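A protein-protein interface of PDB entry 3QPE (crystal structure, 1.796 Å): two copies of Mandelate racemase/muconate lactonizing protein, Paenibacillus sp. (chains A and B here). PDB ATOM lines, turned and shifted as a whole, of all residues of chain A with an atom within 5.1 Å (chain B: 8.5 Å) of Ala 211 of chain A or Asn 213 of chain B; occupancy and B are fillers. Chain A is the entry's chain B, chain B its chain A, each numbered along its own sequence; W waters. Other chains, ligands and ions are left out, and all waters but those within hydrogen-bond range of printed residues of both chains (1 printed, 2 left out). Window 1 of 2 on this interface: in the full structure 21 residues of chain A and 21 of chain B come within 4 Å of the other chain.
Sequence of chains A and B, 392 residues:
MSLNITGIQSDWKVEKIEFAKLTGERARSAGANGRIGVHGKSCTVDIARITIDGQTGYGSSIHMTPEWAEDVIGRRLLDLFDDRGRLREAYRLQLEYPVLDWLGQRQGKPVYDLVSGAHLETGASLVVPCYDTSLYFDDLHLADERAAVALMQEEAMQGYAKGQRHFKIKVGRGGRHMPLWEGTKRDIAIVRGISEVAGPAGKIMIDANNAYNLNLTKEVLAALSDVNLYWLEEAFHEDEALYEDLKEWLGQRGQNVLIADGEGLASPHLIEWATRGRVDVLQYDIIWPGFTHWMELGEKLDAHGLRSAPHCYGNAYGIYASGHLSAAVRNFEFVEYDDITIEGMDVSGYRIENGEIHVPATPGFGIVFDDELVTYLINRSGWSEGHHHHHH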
ATOM      1  N   GLY A  34     -18.162  21.342  12.136  1.00  0.00           N
ATOM      2  CA  GLY A  34     -19.090  20.796  13.113  1.00  0.00           C
ATOM      3  C   GLY A  34     -20.546  21.175  12.891  1.00  0.00           C
ATOM      4  O   GLY A  34     -21.439  20.355  13.105  1.00  0.00           O
ATOM      5  N   VAL A 171     -13.105  19.456  14.487  1.00  0.00           N
ATOM      6  CA  VAL A 171     -13.721  18.285  15.088  1.00  0.00           C
ATOM      7  C   VAL A 171     -15.208  18.556  15.333  1.00  0.00           C
ATOM      8  O   VAL A 171     -15.698  19.652  15.064  1.00  0.00           O
ATOM      9  CB  VAL A 171     -13.016  17.892  16.404  1.00  0.00           C
ATOM     10  CG1 VAL A 171     -11.539  17.630  16.137  1.00  0.00           C
ATOM     11  CG2 VAL A 171     -13.166  18.997  17.456  1.00  0.00           C
ATOM     12  N   GLY A 172     -15.923  17.562  15.852  1.00  0.00           N
ATOM     13  CA  GLY A 172     -17.359  17.690  16.015  1.00  0.00           C
ATOM     14  C   GLY A 172     -18.145  16.941  14.955  1.00  0.00           C
ATOM     15  O   GLY A 172     -19.311  17.231  14.731  1.00  0.00           O
ATOM     16  N   GLY A 174     -19.532  14.163  15.002  1.00  0.00           N
ATOM     17  CA  GLY A 174     -20.707  13.519  15.563  1.00  0.00           C
ATOM     18  C   GLY A 174     -21.852  14.448  15.947  1.00  0.00           C
ATOM     19  O   GLY A 174     -22.968  13.997  16.190  1.00  0.00           O
ATOM     20  N   GLY A 175     -21.585  15.744  15.998  1.00  0.00           N
ATOM     21  CA  GLY A 175     -22.618  16.705  16.323  1.00  0.00           C
ATOM     22  C   GLY A 175     -23.748  16.772  15.314  1.00  0.00           C
ATOM     23  O   GLY A 175     -24.907  16.871  15.691  1.00  0.00           O
ATOM     24  N   LEU A 180     -23.274  10.187  16.373  1.00  0.00           N
ATOM     25  CA  LEU A 180     -22.609  10.857  17.482  1.00  0.00           C
ATOM     26  C   LEU A 180     -21.325  10.169  17.925  1.00  0.00           C
ATOM     27  O   LEU A 180     -20.267  10.796  18.023  1.00  0.00           O
ATOM     28  CB  LEU A 180     -23.567  10.972  18.672  1.00  0.00           C
ATOM     29  CG  LEU A 180     -22.984  11.513  19.979  1.00  0.00           C
ATOM     30  CD1 LEU A 180     -22.627  12.976  19.843  1.00  0.00           C
ATOM     31  CD2 LEU A 180     -23.973  11.307  21.117  1.00  0.00           C
ATOM     32  N   ALA A 208     -14.334  22.639  17.583  1.00  0.00           N
ATOM     33  CA  ALA A 208     -15.554  21.840  17.472  1.00  0.00           C
ATOM     34  C   ALA A 208     -16.706  22.585  16.829  1.00  0.00           C
ATOM     35  O   ALA A 208     -17.747  21.989  16.552  1.00  0.00           O
ATOM     36  CB  ALA A 208     -15.988  21.353  18.838  1.00  0.00           C
ATOM     37  N   ASN A 209     -16.532  23.890  16.622  1.00  0.00           N
ATOM     38  CA  ASN A 209     -17.620  24.743  16.183  1.00  0.00           C
ATOM     39  C   ASN A 209     -18.893  24.457  16.964  1.00  0.00           C
ATOM     40  O   ASN A 209     -19.983  24.315  16.400  1.00  0.00           O
ATOM     41  CB  ASN A 209     -17.833  24.638  14.675  1.00  0.00           C
ATOM     42  CG  ASN A 209     -16.763  25.374  13.898  1.00  0.00           C
ATOM     43  OD1 ASN A 209     -15.831  24.763  13.377  1.00  0.00           O
ATOM     44  ND2 ASN A 209     -16.875  26.697  13.842  1.00  0.00           N
ATOM     45  N   ASN A 210     -18.717  24.382  18.280  1.00  0.00           N
ATOM     46  CA  ASN A 210     -19.794  24.207  19.249  1.00  0.00           C
ATOM     47  C   ASN A 210     -20.525  22.867  19.191  1.00  0.00           C
ATOM     48  O   ASN A 210     -21.549  22.697  19.836  1.00  0.00           O
ATOM     49  CB  ASN A 210     -20.784  25.372  19.183  1.00  0.00           C
ATOM     50  CG  ASN A 210     -20.183  26.668  19.674  1.00  0.00           C
ATOM     51  OD1 ASN A 210     -19.211  26.663  20.432  1.00  0.00           O
ATOM     52  ND2 ASN A 210     -20.753  27.784  19.253  1.00  0.00           N
ATOM     53  N   ALA A 211     -20.004  21.916  18.431  1.00  0.00           N
ATOM     54  CA  ALA A 211     -20.717  20.648  18.257  1.00  0.00           C
ATOM     55  C   ALA A 211     -20.678  19.692  19.464  1.00  0.00           C
ATOM     56  O   ALA A 211     -21.315  18.645  19.414  1.00  0.00           O
ATOM     57  CB  ALA A 211     -20.238  19.912  16.994  1.00  0.00           C
ATOM     58  N   TYR A 212     -19.941  20.029  20.524  1.00  0.00           N
ATOM     59  CA  TYR A 212     -19.845  19.132  21.690  1.00  0.00           C
ATOM     60  C   TYR A 212     -20.723  19.634  22.842  1.00  0.00           C
ATOM     61  O   TYR A 212     -21.363  20.683  22.753  1.00  0.00           O
ATOM     62  CB  TYR A 212     -18.405  19.055  22.212  1.00  0.00           C
ATOM     63  CG  TYR A 212     -17.384  18.347  21.352  1.00  0.00           C
ATOM     64  CD1 TYR A 212     -17.762  17.471  20.356  1.00  0.00           C
ATOM     65  CD2 TYR A 212     -16.025  18.556  21.558  1.00  0.00           C
ATOM     66  CE1 TYR A 212     -16.812  16.818  19.578  1.00  0.00           C
ATOM     67  CE2 TYR A 212     -15.073  17.913  20.796  1.00  0.00           C
ATOM     68  CZ  TYR A 212     -15.467  17.045  19.808  1.00  0.00           C
ATOM     69  OH  TYR A 212     -14.520  16.394  19.042  1.00  0.00           O
ATOM     70  N   ASN A 213     -20.760  18.853  23.918  1.00  0.00           N
ATOM     71  CA  ASN A 213     -21.171  19.350  25.231  1.00  0.00           C
ATOM     72  C   ASN A 213     -20.030  19.067  26.192  1.00  0.00           C
ATOM     73  O   ASN A 213     -19.004  18.526  25.778  1.00  0.00           O
ATOM     74  CB  ASN A 213     -22.499  18.745  25.707  1.00  0.00           C
ATOM     75  CG  ASN A 213     -22.468  17.225  25.817  1.00  0.00           C
ATOM     76  OD1 ASN A 213     -21.408  16.603  25.933  1.00  0.00           O
ATOM     77  ND2 ASN A 213     -23.647  16.620  25.771  1.00  0.00           N
ATOM     78  N   LEU A 216     -18.854  15.252  26.428  1.00  0.00           N
ATOM     79  CA  LEU A 216     -18.302  14.791  25.163  1.00  0.00           C
ATOM     80  C   LEU A 216     -16.908  15.401  25.021  1.00  0.00           C
ATOM     81  O   LEU A 216     -15.966  14.727  24.604  1.00  0.00           O
ATOM     82  CB  LEU A 216     -19.203  15.218  23.998  1.00  0.00           C
ATOM     83  CG  LEU A 216     -19.716  14.173  23.002  1.00  0.00           C
ATOM     84  CD1 LEU A 216     -20.174  14.857  21.711  1.00  0.00           C
ATOM     85  CD2 LEU A 216     -18.680  13.114  22.697  1.00  0.00           C
ATOM     86  N   GLU A 234     -14.056  26.639  20.910  1.00  0.00           N
ATOM     87  CA  GLU A 234     -15.503  26.452  20.810  1.00  0.00           C
ATOM     88  C   GLU A 234     -15.976  24.999  20.964  1.00  0.00           C
ATOM     89  O   GLU A 234     -16.600  24.433  20.063  1.00  0.00           O
ATOM     90  CB  GLU A 234     -16.006  27.030  19.483  1.00  0.00           C
ATOM     91  CG  GLU A 234     -15.718  28.516  19.336  1.00  0.00           C
ATOM     92  CD  GLU A 234     -16.747  29.230  18.473  1.00  0.00           C
ATOM     93  OE1 GLU A 234     -16.848  28.942  17.273  1.00  0.00           O
ATOM     94  OE2 GLU A 234     -17.477  30.068  19.000  1.00  0.00           O
ATOM     95  N   ALA A 235     -15.688  24.396  22.111  1.00  0.00           N
ATOM     96  CA  ALA A 235     -16.183  23.053  22.374  1.00  0.00           C
ATOM     97  C   ALA A 235     -17.704  23.092  22.336  1.00  0.00           C
ATOM     98  O   ALA A 235     -18.352  22.172  21.832  1.00  0.00           O
ATOM     99  CB  ALA A 235     -15.705  22.569  23.736  1.00  0.00           C
ATOM    100  N   GLY B 175     -24.916  15.861  29.936  1.00  0.00           N
ATOM    101  CA  GLY B 175     -24.108  16.983  29.493  1.00  0.00           C
ATOM    102  C   GLY B 175     -22.973  17.268  30.460  1.00  0.00           C
ATOM    103  O   GLY B 175     -21.851  17.549  30.042  1.00  0.00           O
ATOM    104  N   LEU B 180     -22.219  10.642  29.826  1.00  0.00           N
ATOM    105  CA  LEU B 180     -23.083  11.134  28.745  1.00  0.00           C
ATOM    106  C   LEU B 180     -24.105  10.115  28.282  1.00  0.00           C
ATOM    107  O   LEU B 180     -25.283  10.418  28.114  1.00  0.00           O
ATOM    108  CB  LEU B 180     -22.260  11.610  27.542  1.00  0.00           C
ATOM    109  CG  LEU B 180     -23.073  12.141  26.353  1.00  0.00           C
ATOM    110  CD1 LEU B 180     -24.116  13.140  26.801  1.00  0.00           C
ATOM    111  CD2 LEU B 180     -22.153  12.786  25.333  1.00  0.00           C
ATOM    112  N   THR B 184     -28.165  10.383  29.150  1.00  0.00           N
ATOM    113  CA  THR B 184     -29.153  10.504  28.086  1.00  0.00           C
ATOM    114  C   THR B 184     -30.210   9.387  28.152  1.00  0.00           C
ATOM    115  O   THR B 184     -31.405   9.627  27.943  1.00  0.00           O
ATOM    116  CB  THR B 184     -28.469  10.564  26.704  1.00  0.00           C
ATOM    117  OG1 THR B 184     -27.500  11.621  26.708  1.00  0.00           O
ATOM    118  CG2 THR B 184     -29.488  10.816  25.609  1.00  0.00           C
ATOM    119  N   ALA B 208     -33.440  21.333  27.828  1.00  0.00           N
ATOM    120  CA  ALA B 208     -32.101  20.774  27.938  1.00  0.00           C
ATOM    121  C   ALA B 208     -31.099  21.735  28.549  1.00  0.00           C
ATOM    122  O   ALA B 208     -29.978  21.348  28.877  1.00  0.00           O
ATOM    123  CB  ALA B 208     -31.607  20.289  26.552  1.00  0.00           C
ATOM    124  N   ASN B 210     -29.376  23.713  27.067  1.00  0.00           N
ATOM    125  CA  ASN B 210     -28.274  23.793  26.122  1.00  0.00           C
ATOM    126  C   ASN B 210     -27.286  22.649  26.246  1.00  0.00           C
ATOM    127  O   ASN B 210     -26.210  22.673  25.649  1.00  0.00           O
ATOM    128  CB  ASN B 210     -27.567  25.144  26.242  1.00  0.00           C
ATOM    129  CG  ASN B 210     -28.394  26.282  25.650  1.00  0.00           C
ATOM    130  OD1 ASN B 210     -29.255  26.054  24.814  1.00  0.00           O
ATOM    131  ND2 ASN B 210     -28.133  27.504  26.091  1.00  0.00           N
ATOM    132  N   ALA B 211     -27.677  21.629  27.005  1.00  0.00           N
ATOM    133  CA  ALA B 211     -26.803  20.490  27.270  1.00  0.00           C
ATOM    134  C   ALA B 211     -26.662  19.483  26.124  1.00  0.00           C
ATOM    135  O   ALA B 211     -25.803  18.618  26.192  1.00  0.00           O
ATOM    136  CB  ALA B 211     -27.255  19.769  28.556  1.00  0.00           C
ATOM    137  N   TYR B 212     -27.483  19.587  25.082  1.00  0.00           N
ATOM    138  CA  TYR B 212     -27.391  18.638  23.962  1.00  0.00           C
ATOM    139  C   TYR B 212     -26.533  19.188  22.818  1.00  0.00           C
ATOM    140  O   TYR B 212     -26.090  20.333  22.860  1.00  0.00           O
ATOM    141  CB  TYR B 212     -28.786  18.284  23.412  1.00  0.00           C
ATOM    142  CG  TYR B 212     -29.636  17.421  24.302  1.00  0.00           C
ATOM    143  CD1 TYR B 212     -29.064  16.665  25.310  1.00  0.00           C
ATOM    144  CD2 TYR B 212     -31.015  17.337  24.117  1.00  0.00           C
ATOM    145  CE1 TYR B 212     -29.837  15.862  26.123  1.00  0.00           C
ATOM    146  CE2 TYR B 212     -31.796  16.544  24.931  1.00  0.00           C
ATOM    147  CZ  TYR B 212     -31.191  15.799  25.930  1.00  0.00           C
ATOM    148  OH  TYR B 212     -31.940  14.991  26.755  1.00  0.00           O
ATOM    149  N   ASN B 213     -26.279  18.350  21.817  1.00  0.00           N
ATOM    150  CA  ASN B 213     -25.913  18.828  20.482  1.00  0.00           C
ATOM    151  C   ASN B 213     -27.004  18.353  19.510  1.00  0.00           C
ATOM    152  O   ASN B 213     -28.032  17.853  19.956  1.00  0.00           O
ATOM    153  CB  ASN B 213     -24.497  18.399  20.084  1.00  0.00           C
ATOM    154  CG  ASN B 213     -24.328  16.898  20.029  1.00  0.00           C
ATOM    155  OD1 ASN B 213     -25.298  16.164  19.933  1.00  0.00           O
ATOM    156  ND2 ASN B 213     -23.091  16.438  20.078  1.00  0.00           N
ATOM    157  N   LEU B 214     -26.830  18.530  18.201  1.00  0.00           N
ATOM    158  CA  LEU B 214     -27.928  18.222  17.278  1.00  0.00           C
ATOM    159  C   LEU B 214     -28.275  16.724  17.246  1.00  0.00           C
ATOM    160  O   LEU B 214     -29.441  16.352  17.277  1.00  0.00           O
ATOM    161  CB  LEU B 214     -27.630  18.748  15.861  1.00  0.00           C
ATOM    162  CG  LEU B 214     -28.773  18.557  14.862  1.00  0.00           C
ATOM    163  CD1 LEU B 214     -30.085  19.144  15.379  1.00  0.00           C
ATOM    164  CD2 LEU B 214     -28.418  19.123  13.483  1.00  0.00           C
ATOM    165  N   ASN B 215     -27.266  15.861  17.210  1.00  0.00           N
ATOM    166  CA  ASN B 215     -27.536  14.429  17.135  1.00  0.00           C
ATOM    167  C   ASN B 215     -28.033  13.828  18.458  1.00  0.00           C
ATOM    168  O   ASN B 215     -28.836  12.908  18.464  1.00  0.00           O
ATOM    169  CB  ASN B 215     -26.331  13.667  16.573  1.00  0.00           C
ATOM    170  CG  ASN B 215     -26.320  13.651  15.054  1.00  0.00           C
ATOM    171  OD1 ASN B 215     -27.371  13.710  14.421  1.00  0.00           O
ATOM    172  ND2 ASN B 215     -25.131  13.590  14.466  1.00  0.00           N
ATOM    173  N   LEU B 216     -27.565  14.349  19.583  1.00  0.00           N
ATOM    174  CA  LEU B 216     -28.131  13.927  20.863  1.00  0.00           C
ATOM    175  C   LEU B 216     -29.597  14.276  20.888  1.00  0.00           C
ATOM    176  O   LEU B 216     -30.415  13.481  21.324  1.00  0.00           O
ATOM    177  CB  LEU B 216     -27.429  14.604  22.025  1.00  0.00           C
ATOM    178  CG  LEU B 216     -26.186  13.880  22.494  1.00  0.00           C
ATOM    179  CD1 LEU B 216     -25.384  14.805  23.392  1.00  0.00           C
ATOM    180  CD2 LEU B 216     -26.584  12.595  23.240  1.00  0.00           C
ATOM    181  N   THR B 217     -29.921  15.475  20.412  1.00  0.00           N
ATOM    182  CA  THR B 217     -31.305  15.914  20.323  1.00  0.00           C
ATOM    183  C   THR B 217     -32.158  14.963  19.499  1.00  0.00           C
ATOM    184  O   THR B 217     -33.191  14.507  19.962  1.00  0.00           O
ATOM    185  CB  THR B 217     -31.434  17.374  19.785  1.00  0.00           C
ATOM    186  OG1 THR B 217     -30.646  18.245  20.600  1.00  0.00           O
ATOM    187  CG2 THR B 217     -32.876  17.842  19.853  1.00  0.00           C
ATOM    188  N   LYS B 218     -31.737  14.651  18.280  1.00  0.00           N
ATOM    189  CA  LYS B 218     -32.526  13.749  17.449  1.00  0.00           C
ATOM    190  C   LYS B 218     -32.674  12.352  18.078  1.00  0.00           C
ATOM    191  O   LYS B 218     -33.721  11.715  17.946  1.00  0.00           O
ATOM    192  CB  LYS B 218     -31.923  13.646  16.047  1.00  0.00           C
ATOM    193  CG  LYS B 218     -31.825  14.970  15.312  1.00  0.00           C
ATOM    194  CD  LYS B 218     -31.021  14.796  14.017  1.00  0.00           C
ATOM    195  CE  LYS B 218     -31.313  15.909  13.029  1.00  0.00           C
ATOM    196  NZ  LYS B 218     -30.416  15.837  11.839  1.00  0.00           N
ATOM    197  N   GLU B 219     -31.631  11.871  18.736  1.00  0.00           N
ATOM    198  CA  GLU B 219     -31.704  10.560  19.384  1.00  0.00           C
ATOM    199  C   GLU B 219     -32.806  10.576  20.436  1.00  0.00           C
ATOM    200  O   GLU B 219     -33.644   9.677  20.494  1.00  0.00           O
ATOM    201  CB  GLU B 219     -30.359  10.174  19.999  1.00  0.00           C
ATOM    202  CG  GLU B 219     -30.390   8.916  20.842  1.00  0.00           C
ATOM    203  CD  GLU B 219     -29.002   8.456  21.251  1.00  0.00           C
ATOM    204  OE1 GLU B 219     -28.088   8.469  20.394  1.00  0.00           O
ATOM    205  OE2 GLU B 219     -28.823   8.089  22.431  1.00  0.00           O
ATOM    206  N   VAL B 220     -32.827  11.629  21.247  1.00  0.00           N
ATOM    207  CA  VAL B 220     -33.800  11.744  22.328  1.00  0.00           C
ATOM    208  C   VAL B 220     -35.211  11.881  21.787  1.00  0.00           C
ATOM    209  O   VAL B 220     -36.136  11.246  22.282  1.00  0.00           O
ATOM    210  CB  VAL B 220     -33.475  12.929  23.242  1.00  0.00           C
ATOM    211  CG1 VAL B 220     -34.617  13.198  24.194  1.00  0.00           C
ATOM    212  CG2 VAL B 220     -32.187  12.652  24.004  1.00  0.00           C
ATOM    213  N   LEU B 221     -35.373  12.716  20.766  1.00  0.00           N
ATOM    214  CA  LEU B 221     -36.678  12.936  20.164  1.00  0.00           C
ATOM    215  C   LEU B 221     -37.227  11.662  19.518  1.00  0.00           C
ATOM    216  O   LEU B 221     -38.413  11.359  19.640  1.00  0.00           O
ATOM    217  CB  LEU B 221     -36.589  14.037  19.109  1.00  0.00           C
ATOM    218  CG  LEU B 221     -36.259  15.435  19.630  1.00  0.00           C
ATOM    219  CD1 LEU B 221     -36.146  16.395  18.473  1.00  0.00           C
ATOM    220  CD2 LEU B 221     -37.317  15.901  20.603  1.00  0.00           C
ATOM    221  N   LEU B 232     -39.689  21.509  22.518  1.00  0.00           N
ATOM    222  CA  LEU B 232     -38.302  21.289  22.864  1.00  0.00           C
ATOM    223  C   LEU B 232     -37.648  22.629  23.111  1.00  0.00           C
ATOM    224  O   LEU B 232     -37.563  23.453  22.201  1.00  0.00           O
ATOM    225  CB  LEU B 232     -37.583  20.566  21.714  1.00  0.00           C
ATOM    226  CG  LEU B 232     -36.068  20.393  21.848  1.00  0.00           C
ATOM    227  CD1 LEU B 232     -35.654  19.489  23.043  1.00  0.00           C
ATOM    228  CD2 LEU B 232     -35.491  19.866  20.529  1.00  0.00           C
ATOM    229  N   GLU B 234     -34.433  25.013  24.376  1.00  0.00           N
ATOM    230  CA  GLU B 234     -32.984  25.123  24.523  1.00  0.00           C
ATOM    231  C   GLU B 234     -32.221  23.792  24.425  1.00  0.00           C
ATOM    232  O   GLU B 234     -31.426  23.463  25.299  1.00  0.00           O
ATOM    233  CB  GLU B 234     -32.619  25.841  25.826  1.00  0.00           C
ATOM    234  CG  GLU B 234     -33.111  27.289  25.894  1.00  0.00           C
ATOM    235  CD  GLU B 234     -32.190  28.184  26.731  1.00  0.00           C
ATOM    236  OE1 GLU B 234     -31.978  27.919  27.927  1.00  0.00           O
ATOM    237  OE2 GLU B 234     -31.665  29.170  26.200  1.00  0.00           O
ATOM    238  N   ALA B 235     -32.442  23.049  23.346  1.00  0.00           N
ATOM    239  CA  ALA B 235     -31.681  21.820  23.123  1.00  0.00           C
ATOM    240  C   ALA B 235     -30.188  22.139  23.159  1.00  0.00           C
ATOM    241  O   ALA B 235     -29.395  21.410  23.736  1.00  0.00           O
ATOM    242  CB  ALA B 235     -32.061  21.197  21.778  1.00  0.00           C
ATOM    243  N   PHE B 236     -29.822  23.260  22.540  1.00  0.00           N
ATOM    244  CA  PHE B 236     -28.436  23.702  22.426  1.00  0.00           C
ATOM    245  C   PHE B 236     -28.506  25.207  22.138  1.00  0.00           C
ATOM    246  O   PHE B 236     -29.572  25.725  21.785  1.00  0.00           O
ATOM    247  CB  PHE B 236     -27.727  22.960  21.281  1.00  0.00           C
ATOM    248  CG  PHE B 236     -28.594  22.761  20.078  1.00  0.00           C
ATOM    249  CD1 PHE B 236     -29.128  21.520  19.791  1.00  0.00           C
ATOM    250  CD2 PHE B 236     -28.917  23.830  19.256  1.00  0.00           C
ATOM    251  CE1 PHE B 236     -29.951  21.332  18.695  1.00  0.00           C
ATOM    252  CE2 PHE B 236     -29.737  23.647  18.164  1.00  0.00           C
ATOM    253  CZ  PHE B 236     -30.253  22.402  17.876  1.00  0.00           C
ATOM    254  N   HIS B 237     -27.411  25.931  22.324  1.00  0.00           N
ATOM    255  CA  HIS B 237     -27.514  27.371  22.149  1.00  0.00           C
ATOM    256  C   HIS B 237     -28.006  27.676  20.735  1.00  0.00           C
ATOM    257  O   HIS B 237     -27.496  27.117  19.768  1.00  0.00           O
ATOM    258  CB  HIS B 237     -26.190  28.081  22.404  1.00  0.00           C
ATOM    259  CG  HIS B 237     -26.295  29.563  22.259  1.00  0.00           C
ATOM    260  ND1 HIS B 237     -27.144  30.318  23.037  1.00  0.00           N
ATOM    261  CD2 HIS B 237     -25.714  30.423  21.390  1.00  0.00           C
ATOM    262  CE1 HIS B 237     -27.059  31.586  22.674  1.00  0.00           C
ATOM    263  NE2 HIS B 237     -26.200  31.676  21.672  1.00  0.00           N
ATOM    264  N   ASP B 239     -28.964  28.499  17.075  1.00  0.00           N
ATOM    265  CA  ASP B 239     -28.109  28.512  15.894  1.00  0.00           C
ATOM    266  C   ASP B 239     -29.058  28.256  14.723  1.00  0.00           C
ATOM    267  O   ASP B 239     -29.724  27.221  14.678  1.00  0.00           O
ATOM    268  CB  ASP B 239     -27.064  27.402  16.019  1.00  0.00           C
ATOM    269  CG  ASP B 239     -26.133  27.313  14.825  1.00  0.00           C
ATOM    270  OD1 ASP B 239     -26.594  27.550  13.692  1.00  0.00           O
ATOM    271  OD2 ASP B 239     -24.934  26.993  15.022  1.00  0.00           O
ATOM    272  N   LEU B 242     -28.592  24.975  12.668  1.00  0.00           N
ATOM    273  CA  LEU B 242     -28.929  23.751  13.380  1.00  0.00           C
ATOM    274  C   LEU B 242     -30.438  23.604  13.527  1.00  0.00           C
ATOM    275  O   LEU B 242     -30.964  22.519  13.339  1.00  0.00           O
ATOM    276  CB  LEU B 242     -28.225  23.650  14.740  1.00  0.00           C
ATOM    277  CG  LEU B 242     -26.693  23.617  14.712  1.00  0.00           C
ATOM    278  CD1 LEU B 242     -26.122  23.552  16.095  1.00  0.00           C
ATOM    279  CD2 LEU B 242     -26.206  22.430  13.871  1.00  0.00           C
ATOM    280  N   LEU B 246     -32.954  20.757  12.211  1.00  0.00           N
ATOM    281  CA  LEU B 246     -33.880  20.072  13.118  1.00  0.00           C
ATOM    282  C   LEU B 246     -35.341  20.164  12.668  1.00  0.00           C
ATOM    283  O   LEU B 246     -36.060  19.162  12.683  1.00  0.00           O
ATOM    284  CB  LEU B 246     -33.715  20.558  14.567  1.00  0.00           C
ATOM    285  CG  LEU B 246     -34.456  19.769  15.656  1.00  0.00           C
ATOM    286  CD1 LEU B 246     -34.074  18.292  15.648  1.00  0.00           C
ATOM    287  CD2 LEU B 246     -34.167  20.372  17.029  1.00  0.00           C
HETATM  288  O   HOH W   1     -23.384  27.584  17.605  1.00  0.00           O
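The side-chain amide nitrogen of Asn 213 of chain A is in hydrogen-bond range of the backbone carbonyl oxygen of Ala 211 of chain B, at 3.0 Å.
The backbone carbonyl oxygen (O) of Ala 211 of chain A is in hydrogen-bond range of the side-chain amide nitrogen (ND2) of Asn 213 of chain B (2.9 Å).
ND2 of Asn 215 of chain B is in hydrogen-bond range of O of Gly 174 of chain A.
O of Gly 175 of chain A sits at hydrogen-bond distance from N of Asn 215 of chain B (3.0 Å).
OG1 of Thr 184 of chain B sits at hydrogen-bond distance from O of Leu 180 of chain B (2.9 Å).
The side-chain amide oxygen (OD1) of Asn 213 of chain B sits at hydrogen-bond distance from the backbone NH (N) of Asn 215 of chain B.
OD1 of Asn 213 of chain B lies within hydrogen-bond range of N of Leu 216 of chain B, at 2.9 Å.
OG1 of Thr 217 of chain B sits at hydrogen-bond distance from O of Asn 213 of chain B (2.7 Å).
N of Leu 216 of chain A is in hydrogen-bond range of OD1 of Asn 213 of chain A, 2.9 Å away.
Among the printed residues, merely in contact across the chains: Gly 175 of chain A with Leu 214 of chain B, Asn 213 of chain A with Leu 216 of chain B, Leu 180 of chain A with Asn 213 of chain B, Leu 180 of chain A with Leu 216 of chain B, Leu 216 of chain A with Leu 180 of chain B, Asn 213 of chain A with Leu 180 of chain B, Leu 216 of chain A with Asn 213 of chain B, Asn 213 of chain A with Gly 175 of chain B and Gly 175 of chain A with Asn 213 of chain B.
Printed residues of chain B within 4 Å of Gly 175 of chain A: Asn 213, Leu 214 and Asn 215.
Of the printed residues of chain B, Ala 211 of chain A touches Asn 213 (2.9 Å).
Of the printed residues of chain A, Ala 211 of chain B touches Asn 213 (3.0 Å).
Asn 213 of chain B touches four residues of chain A.
The nearest residue of chain B that does not touch Ala 211 of chain A is Leu 214 of chain B (5.6 Å).
The nearest residue of chain A that does not touch Asn 213 of chain B is Tyr 212 of chain A (4.5 Å).
The nearest printed residue of chain A that does not touch Asn 215 of chain B is Leu 180 of chain A (4.3 Å).
Hydrophobic or aromatic side chains of chain B that line the printed part of chain A: Leu 180, Leu 214 and Leu 216.
Hydrophobic or aromatic side chains of chain A that line the printed part of chain B: Leu 180 and Leu 216.
Gly 175 of chain A touches Asn 213 of chain B, and with the chains exchanged Asn 213 of chain A touches Gly 175 of chain B.
Leu 180 of chain A touches Asn 213 of chain B, and with the chains exchanged Asn 213 of chain A touches Leu 180 of chain B.
Leu 180 of chain A touches Leu 216 of chain B, and with the chains exchanged Leu 216 of chain A touches Leu 180 of chain B.
Asn 213 of chain A touches Leu 216 of chain B, and with the chains exchanged Leu 216 of chain A touches Asn 213 of chain B.
Of the 13 pairs that touch across the chains among the printed residues, 10 have their exchanged pair printed and touching as well.
Water W1 bridges OD2 of Asp 239 of chain B (3.1 Å) and ND2 of Asn 210 of chain A (3.1 Å).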
